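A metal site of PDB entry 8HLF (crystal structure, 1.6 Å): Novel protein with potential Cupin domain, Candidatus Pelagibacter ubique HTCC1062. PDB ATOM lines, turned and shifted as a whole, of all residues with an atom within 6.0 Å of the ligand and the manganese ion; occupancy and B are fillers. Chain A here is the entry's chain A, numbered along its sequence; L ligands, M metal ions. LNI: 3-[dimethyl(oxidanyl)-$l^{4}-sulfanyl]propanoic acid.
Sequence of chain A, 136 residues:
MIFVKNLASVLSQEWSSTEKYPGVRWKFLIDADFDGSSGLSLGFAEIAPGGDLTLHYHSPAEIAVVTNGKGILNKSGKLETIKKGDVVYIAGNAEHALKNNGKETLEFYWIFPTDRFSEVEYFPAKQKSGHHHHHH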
ATOM      1  N   TYR A  21     -31.086   6.298 -17.047  1.00  0.00           N
ATOM      2  CA  TYR A  21     -30.600   7.434 -17.827  1.00  0.00           C
ATOM      3  C   TYR A  21     -31.601   8.580 -17.684  1.00  0.00           C
ATOM      4  O   TYR A  21     -32.468   8.776 -18.541  1.00  0.00           O
ATOM      5  CB  TYR A  21     -30.408   7.071 -19.306  1.00  0.00           C
ATOM      6  CG  TYR A  21     -29.440   5.935 -19.548  1.00  0.00           C
ATOM      7  CD1 TYR A  21     -28.325   5.744 -18.719  1.00  0.00           C
ATOM      8  CD2 TYR A  21     -29.615   5.060 -20.611  1.00  0.00           C
ATOM      9  CE1 TYR A  21     -27.445   4.699 -18.941  1.00  0.00           C
ATOM     10  CE2 TYR A  21     -28.734   4.011 -20.842  1.00  0.00           C
ATOM     11  CZ  TYR A  21     -27.643   3.844 -20.011  1.00  0.00           C
ATOM     12  OH  TYR A  21     -26.768   2.811 -20.238  1.00  0.00           O
ATOM     13  N   VAL A  24     -33.164  11.290 -20.540  1.00  0.00           N
ATOM     14  CA  VAL A  24     -32.771  10.772 -21.845  1.00  0.00           C
ATOM     15  C   VAL A  24     -33.970  10.052 -22.462  1.00  0.00           C
ATOM     16  O   VAL A  24     -34.623   9.243 -21.793  1.00  0.00           O
ATOM     17  CB  VAL A  24     -31.565   9.818 -21.740  1.00  0.00           C
ATOM     18  CG1 VAL A  24     -31.134   9.328 -23.124  1.00  0.00           C
ATOM     19  CG2 VAL A  24     -30.390  10.517 -21.033  1.00  0.00           C
ATOM     20  N   ARG A  25     -34.254  10.345 -23.733  1.00  0.00           N
ATOM     21  CA  ARG A  25     -35.308   9.647 -24.442  1.00  0.00           C
ATOM     22  C   ARG A  25     -34.893   9.495 -25.900  1.00  0.00           C
ATOM     23  O   ARG A  25     -34.083  10.277 -26.415  1.00  0.00           O
ATOM     24  CB  ARG A  25     -36.658  10.363 -24.336  1.00  0.00           C
ATOM     25  CG  ARG A  25     -36.715  11.741 -24.962  1.00  0.00           C
ATOM     26  CD  ARG A  25     -38.087  12.343 -24.811  1.00  0.00           C
ATOM     27  NE  ARG A  25     -38.251  13.513 -25.663  1.00  0.00           N
ATOM     28  CZ  ARG A  25     -39.392  14.185 -25.782  1.00  0.00           C
ATOM     29  NH1 ARG A  25     -39.460  15.237 -26.580  1.00  0.00           N
ATOM     30  NH2 ARG A  25     -40.456  13.804 -25.091  1.00  0.00           N
ATOM     31  N   TRP A  26     -35.428   8.476 -26.563  1.00  0.00           N
ATOM     32  CA  TRP A  26     -34.963   8.174 -27.909  1.00  0.00           C
ATOM     33  C   TRP A  26     -36.060   7.510 -28.726  1.00  0.00           C
ATOM     34  O   TRP A  26     -37.035   6.975 -28.202  1.00  0.00           O
ATOM     35  CB  TRP A  26     -33.721   7.270 -27.890  1.00  0.00           C
ATOM     36  CG  TRP A  26     -33.891   5.986 -27.130  1.00  0.00           C
ATOM     37  CD1 TRP A  26     -34.262   4.766 -27.637  1.00  0.00           C
ATOM     38  CD2 TRP A  26     -33.664   5.777 -25.731  1.00  0.00           C
ATOM     39  NE1 TRP A  26     -34.286   3.824 -26.637  1.00  0.00           N
ATOM     40  CE2 TRP A  26     -33.926   4.421 -25.457  1.00  0.00           C
ATOM     41  CE3 TRP A  26     -33.261   6.612 -24.685  1.00  0.00           C
ATOM     42  CZ2 TRP A  26     -33.809   3.876 -24.182  1.00  0.00           C
ATOM     43  CZ3 TRP A  26     -33.153   6.071 -23.412  1.00  0.00           C
ATOM     44  CH2 TRP A  26     -33.419   4.719 -23.170  1.00  0.00           C
ATOM     45  N   PHE A  28     -36.309   5.050 -32.586  1.00  0.00           N
ATOM     46  CA  PHE A  28     -35.603   4.235 -33.561  1.00  0.00           C
ATOM     47  C   PHE A  28     -36.075   4.599 -34.959  1.00  0.00           C
ATOM     48  O   PHE A  28     -37.254   4.451 -35.279  1.00  0.00           O
ATOM     49  CB  PHE A  28     -35.848   2.760 -33.280  1.00  0.00           C
ATOM     50  CG  PHE A  28     -35.560   2.381 -31.868  1.00  0.00           C
ATOM     51  CD1 PHE A  28     -34.253   2.241 -31.441  1.00  0.00           C
ATOM     52  CD2 PHE A  28     -36.579   2.187 -30.959  1.00  0.00           C
ATOM     53  CE1 PHE A  28     -33.963   1.898 -30.134  1.00  0.00           C
ATOM     54  CE2 PHE A  28     -36.298   1.848 -29.654  1.00  0.00           C
ATOM     55  CZ  PHE A  28     -34.980   1.699 -29.244  1.00  0.00           C
ATOM     56  N   PHE A  44     -32.488   8.356 -32.790  1.00  0.00           N
ATOM     57  CA  PHE A  44     -32.389   9.775 -32.454  1.00  0.00           C
ATOM     58  C   PHE A  44     -32.647   9.919 -30.974  1.00  0.00           C
ATOM     59  O   PHE A  44     -33.620   9.359 -30.454  1.00  0.00           O
ATOM     60  CB  PHE A  44     -33.398  10.607 -33.243  1.00  0.00           C
ATOM     61  CG  PHE A  44     -33.397  12.065 -32.884  1.00  0.00           C
ATOM     62  CD1 PHE A  44     -32.353  12.890 -33.272  1.00  0.00           C
ATOM     63  CD2 PHE A  44     -34.442  12.606 -32.140  1.00  0.00           C
ATOM     64  CE1 PHE A  44     -32.354  14.254 -32.926  1.00  0.00           C
ATOM     65  CE2 PHE A  44     -34.442  13.965 -31.813  1.00  0.00           C
ATOM     66  CZ  PHE A  44     -33.402  14.781 -32.199  1.00  0.00           C
ATOM     67  N   ALA A  45     -31.779  10.660 -30.289  1.00  0.00           N
ATOM     68  CA  ALA A  45     -31.856  10.805 -28.840  1.00  0.00           C
ATOM     69  C   ALA A  45     -31.910  12.272 -28.455  1.00  0.00           C
ATOM     70  O   ALA A  45     -31.275  13.112 -29.083  1.00  0.00           O
ATOM     71  CB  ALA A  45     -30.666  10.134 -28.153  1.00  0.00           C
ATOM     72  N   LEU A  53     -26.627  10.485 -19.713  1.00  0.00           N
ATOM     73  CA  LEU A  53     -26.418   9.130 -20.217  1.00  0.00           C
ATOM     74  C   LEU A  53     -25.155   8.636 -19.548  1.00  0.00           C
ATOM     75  O   LEU A  53     -24.042   8.998 -19.947  1.00  0.00           O
ATOM     76  CB  LEU A  53     -26.318   9.148 -21.736  1.00  0.00           C
ATOM     77  CG  LEU A  53     -25.975   7.842 -22.456  1.00  0.00           C
ATOM     78  CD1 LEU A  53     -26.974   6.766 -22.083  1.00  0.00           C
ATOM     79  CD2 LEU A  53     -25.967   8.076 -23.953  1.00  0.00           C
ATOM     80  N   HIS A  56     -20.976   3.831 -19.661  1.00  0.00           N
ATOM     81  CA  HIS A  56     -21.382   2.501 -20.095  1.00  0.00           C
ATOM     82  C   HIS A  56     -20.526   2.101 -21.282  1.00  0.00           C
ATOM     83  O   HIS A  56     -19.752   2.895 -21.814  1.00  0.00           O
ATOM     84  CB  HIS A  56     -22.876   2.465 -20.480  1.00  0.00           C
ATOM     85  CG  HIS A  56     -23.162   3.187 -21.756  1.00  0.00           C
ATOM     86  ND1 HIS A  56     -23.399   4.551 -21.791  1.00  0.00           N
ATOM     87  CD2 HIS A  56     -23.230   2.759 -23.033  1.00  0.00           C
ATOM     88  CE1 HIS A  56     -23.613   4.921 -23.039  1.00  0.00           C
ATOM     89  NE2 HIS A  56     -23.508   3.864 -23.819  1.00  0.00           N
ATOM     90  N   TYR A  57     -20.661   0.840 -21.679  1.00  0.00           N
ATOM     91  CA  TYR A  57     -19.992   0.375 -22.878  1.00  0.00           C
ATOM     92  C   TYR A  57     -20.832  -0.737 -23.511  1.00  0.00           C
ATOM     93  O   TYR A  57     -21.728  -1.303 -22.889  1.00  0.00           O
ATOM     94  CB  TYR A  57     -18.570  -0.118 -22.598  1.00  0.00           C
ATOM     95  CG  TYR A  57     -18.461  -1.310 -21.670  1.00  0.00           C
ATOM     96  CD1 TYR A  57     -18.493  -1.137 -20.289  1.00  0.00           C
ATOM     97  CD2 TYR A  57     -18.312  -2.592 -22.169  1.00  0.00           C
ATOM     98  CE1 TYR A  57     -18.389  -2.213 -19.439  1.00  0.00           C
ATOM     99  CE2 TYR A  57     -18.207  -3.689 -21.312  1.00  0.00           C
ATOM    100  CZ  TYR A  57     -18.244  -3.485 -19.952  1.00  0.00           C
ATOM    101  OH  TYR A  57     -18.142  -4.555 -19.083  1.00  0.00           O
ATOM    102  N   HIS A  58     -20.501  -1.031 -24.762  1.00  0.00           N
ATOM    103  CA  HIS A  58     -21.132  -2.094 -25.533  1.00  0.00           C
ATOM    104  C   HIS A  58     -20.175  -2.523 -26.621  1.00  0.00           C
ATOM    105  O   HIS A  58     -19.347  -1.722 -27.078  1.00  0.00           O
ATOM    106  CB  HIS A  58     -22.464  -1.630 -26.134  1.00  0.00           C
ATOM    107  CG  HIS A  58     -22.495  -0.174 -26.437  1.00  0.00           C
ATOM    108  ND1 HIS A  58     -21.617   0.419 -27.319  1.00  0.00           N
ATOM    109  CD2 HIS A  58     -23.296   0.825 -25.975  1.00  0.00           C
ATOM    110  CE1 HIS A  58     -21.853   1.722 -27.367  1.00  0.00           C
ATOM    111  NE2 HIS A  58     -22.868   1.983 -26.566  1.00  0.00           N
ATOM    112  N   GLU A  62     -19.602   2.726 -32.221  1.00  0.00           N
ATOM    113  CA  GLU A  62     -20.760   3.604 -32.278  1.00  0.00           C
ATOM    114  C   GLU A  62     -20.329   4.952 -32.833  1.00  0.00           C
ATOM    115  O   GLU A  62     -19.230   5.432 -32.546  1.00  0.00           O
ATOM    116  CB  GLU A  62     -21.386   3.801 -30.879  1.00  0.00           C
ATOM    117  CG  GLU A  62     -22.584   4.755 -30.847  1.00  0.00           C
ATOM    118  CD  GLU A  62     -23.046   5.098 -29.430  1.00  0.00           C
ATOM    119  OE1 GLU A  62     -22.690   4.382 -28.465  1.00  0.00           O
ATOM    120  OE2 GLU A  62     -23.752   6.118 -29.262  1.00  0.00           O
ATOM    121  N   ILE A  90     -16.901   6.170 -31.142  1.00  0.00           N
ATOM    122  CA  ILE A  90     -16.705   5.462 -29.875  1.00  0.00           C
ATOM    123  C   ILE A  90     -16.331   4.022 -30.217  1.00  0.00           C
ATOM    124  O   ILE A  90     -17.160   3.265 -30.738  1.00  0.00           O
ATOM    125  CB  ILE A  90     -17.967   5.494 -28.998  1.00  0.00           C
ATOM    126  CG1 ILE A  90     -18.383   6.947 -28.757  1.00  0.00           C
ATOM    127  CG2 ILE A  90     -17.729   4.741 -27.705  1.00  0.00           C
ATOM    128  CD1 ILE A  90     -19.854   7.123 -28.629  1.00  0.00           C
ATOM    129  N   HIS A  96     -17.983   5.218 -22.072  1.00  0.00           N
ATOM    130  CA  HIS A  96     -18.354   6.577 -22.460  1.00  0.00           C
ATOM    131  C   HIS A  96     -19.641   7.009 -21.770  1.00  0.00           C
ATOM    132  O   HIS A  96     -20.457   6.190 -21.359  1.00  0.00           O
ATOM    133  CB  HIS A  96     -18.496   6.726 -23.981  1.00  0.00           C
ATOM    134  CG  HIS A  96     -19.483   5.777 -24.589  1.00  0.00           C
ATOM    135  ND1 HIS A  96     -19.254   4.416 -24.681  1.00  0.00           N
ATOM    136  CD2 HIS A  96     -20.710   5.989 -25.117  1.00  0.00           C
ATOM    137  CE1 HIS A  96     -20.295   3.839 -25.259  1.00  0.00           C
ATOM    138  NE2 HIS A  96     -21.192   4.775 -25.539  1.00  0.00           N
ATOM    139  N   PHE A 108     -28.980  14.208 -30.703  1.00  0.00           N
ATOM    140  CA  PHE A 108     -28.037  13.539 -31.582  1.00  0.00           C
ATOM    141  C   PHE A 108     -28.648  12.279 -32.176  1.00  0.00           C
ATOM    142  O   PHE A 108     -29.539  11.655 -31.589  1.00  0.00           O
ATOM    143  CB  PHE A 108     -26.732  13.180 -30.847  1.00  0.00           C
ATOM    144  CG  PHE A 108     -26.905  12.278 -29.659  1.00  0.00           C
ATOM    145  CD1 PHE A 108     -27.264  12.792 -28.435  1.00  0.00           C
ATOM    146  CD2 PHE A 108     -26.676  10.910 -29.770  1.00  0.00           C
ATOM    147  CE1 PHE A 108     -27.430  11.956 -27.319  1.00  0.00           C
ATOM    148  CE2 PHE A 108     -26.819  10.073 -28.663  1.00  0.00           C
ATOM    149  CZ  PHE A 108     -27.201  10.608 -27.446  1.00  0.00           C
ATOM    150  N   TRP A 110     -27.517   8.380 -33.174  1.00  0.00           N
ATOM    151  CA  TRP A 110     -26.484   7.374 -33.011  1.00  0.00           C
ATOM    152  C   TRP A 110     -26.615   6.343 -34.117  1.00  0.00           C
ATOM    153  O   TRP A 110     -27.700   6.150 -34.690  1.00  0.00           O
ATOM    154  CB  TRP A 110     -26.553   6.676 -31.648  1.00  0.00           C
ATOM    155  CG  TRP A 110     -27.591   5.616 -31.565  1.00  0.00           C
ATOM    156  CD1 TRP A 110     -27.480   4.315 -31.955  1.00  0.00           C
ATOM    157  CD2 TRP A 110     -28.914   5.768 -31.043  1.00  0.00           C
ATOM    158  NE1 TRP A 110     -28.645   3.638 -31.714  1.00  0.00           N
ATOM    159  CE2 TRP A 110     -29.558   4.510 -31.157  1.00  0.00           C
ATOM    160  CE3 TRP A 110     -29.643   6.842 -30.516  1.00  0.00           C
ATOM    161  CZ2 TRP A 110     -30.866   4.296 -30.743  1.00  0.00           C
ATOM    162  CZ3 TRP A 110     -30.946   6.638 -30.104  1.00  0.00           C
ATOM    163  CH2 TRP A 110     -31.544   5.361 -30.210  1.00  0.00           C
ATOM    164  N   PHE A 112     -25.103   2.298 -35.067  1.00  0.00           N
ATOM    165  CA  PHE A 112     -24.380   1.080 -34.743  1.00  0.00           C
ATOM    166  C   PHE A 112     -24.244   0.236 -36.006  1.00  0.00           C
ATOM    167  O   PHE A 112     -25.127   0.257 -36.863  1.00  0.00           O
ATOM    168  CB  PHE A 112     -25.126   0.235 -33.702  1.00  0.00           C
ATOM    169  CG  PHE A 112     -25.057   0.755 -32.296  1.00  0.00           C
ATOM    170  CD1 PHE A 112     -23.843   0.775 -31.609  1.00  0.00           C
ATOM    171  CD2 PHE A 112     -26.202   1.169 -31.645  1.00  0.00           C
ATOM    172  CE1 PHE A 112     -23.793   1.231 -30.300  1.00  0.00           C
ATOM    173  CE2 PHE A 112     -26.151   1.625 -30.335  1.00  0.00           C
ATOM    174  CZ  PHE A 112     -24.928   1.656 -29.673  1.00  0.00           C
ATOM    175  N   PHE A 117     -31.147  -2.188 -32.741  1.00  0.00           N
ATOM    176  CA  PHE A 117     -30.698  -1.719 -31.433  1.00  0.00           C
ATOM    177  C   PHE A 117     -30.688  -2.842 -30.416  1.00  0.00           C
ATOM    178  O   PHE A 117     -29.812  -2.903 -29.548  1.00  0.00           O
ATOM    179  CB  PHE A 117     -31.608  -0.580 -30.968  1.00  0.00           C
ATOM    180  CG  PHE A 117     -31.236   0.008 -29.638  1.00  0.00           C
ATOM    181  CD1 PHE A 117     -30.130   0.814 -29.513  1.00  0.00           C
ATOM    182  CD2 PHE A 117     -32.026  -0.230 -28.523  1.00  0.00           C
ATOM    183  CE1 PHE A 117     -29.791   1.373 -28.302  1.00  0.00           C
ATOM    184  CE2 PHE A 117     -31.701   0.327 -27.302  1.00  0.00           C
ATOM    185  CZ  PHE A 117     -30.586   1.126 -27.185  1.00  0.00           C
ATOM    186  N   TYR A 122     -25.855  -3.407 -23.408  1.00  0.00           N
ATOM    187  CA  TYR A 122     -25.229  -2.334 -22.651  1.00  0.00           C
ATOM    188  C   TYR A 122     -24.723  -2.830 -21.305  1.00  0.00           C
ATOM    189  O   TYR A 122     -25.395  -3.550 -20.632  1.00  0.00           O
ATOM    190  CB  TYR A 122     -26.172  -1.163 -22.408  1.00  0.00           C
ATOM    191  CG  TYR A 122     -26.410  -0.219 -23.582  1.00  0.00           C
ATOM    192  CD1 TYR A 122     -26.859  -0.690 -24.775  1.00  0.00           C
ATOM    193  CD2 TYR A 122     -26.222   1.133 -23.462  1.00  0.00           C
ATOM    194  CE1 TYR A 122     -27.069   0.148 -25.800  1.00  0.00           C
ATOM    195  CE2 TYR A 122     -26.433   1.989 -24.502  1.00  0.00           C
ATOM    196  CZ  TYR A 122     -26.880   1.478 -25.672  1.00  0.00           C
ATOM    197  OH  TYR A 122     -27.078   2.282 -26.717  1.00  0.00           O
HETATM  198  O01 LNI L   1     -24.465   6.147 -26.622  1.00  0.00           O
HETATM  199  C01 LNI L   1     -25.391   5.304 -26.797  1.00  0.00           C
HETATM  200  C02 LNI L   1     -26.843   5.765 -26.870  1.00  0.00           C
HETATM  201  O02 LNI L   1     -25.108   4.087 -26.930  1.00  0.00           O
HETATM  202  C03 LNI L   1     -27.660   5.028 -25.804  1.00  0.00           C
HETATM  203  S01 LNI L   1     -29.428   5.185 -26.180  1.00  0.00           S
HETATM  204  C04 LNI L   1     -29.841   4.144 -27.615  1.00  0.00           C
HETATM  205  C05 LNI L   1     -29.815   6.917 -26.558  1.00  0.00           C
HETATM  206  O03 LNI L   1     -30.215   4.752 -25.027  1.00  0.00           O
HETATM  207 MN    MN M   1     -23.177   4.085 -26.098  1.00  0.00          MN
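The side-chain hydroxyl (OH) of Tyr 122 lies close to an oxygen (O02) of the ligand (2.7 Å).
N of Ile 90 lies within hydrogen-bond range of O of Glu 62 (2.8 Å).
N of Ala 45 is in hydrogen-bond range of O of Phe 108 (2.8 Å).
Residues that only touch the ligand: Phe 117 (2.9 Å), Trp 110 (3.3 Å), Trp 26 (3.6 Å), Leu 53 (3.6 Å), Phe 112 (3.7 Å) and Ala 45 (3.7 Å).
Hydrophobic or aromatic side chains that line the ligand: Trp 26, Ala 45, Leu 53, His 56, His 58, Trp 110, Phe 112, Phe 117 and Tyr 122.
Four residues have an atom within 4 Å of the manganese ion: His 56, His 58, Glu 62 and His 96.
An oxygen (O02) of the ligand binds the manganese ion (2.1 Å).
NE2 of His 96 is bound to the manganese ion (2.2 Å).
NE2 of His 58 is bound to the manganese ion, 2.2 Å away.
The manganese ion is bound by a ring nitrogen (NE2) of His 56 (2.3 Å).
The manganese ion is bound by the side-chain carboxylate (OE1) of Glu 62, at 2.4 Å.
O01 of the ligand binds the manganese ion (2.5 Å).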
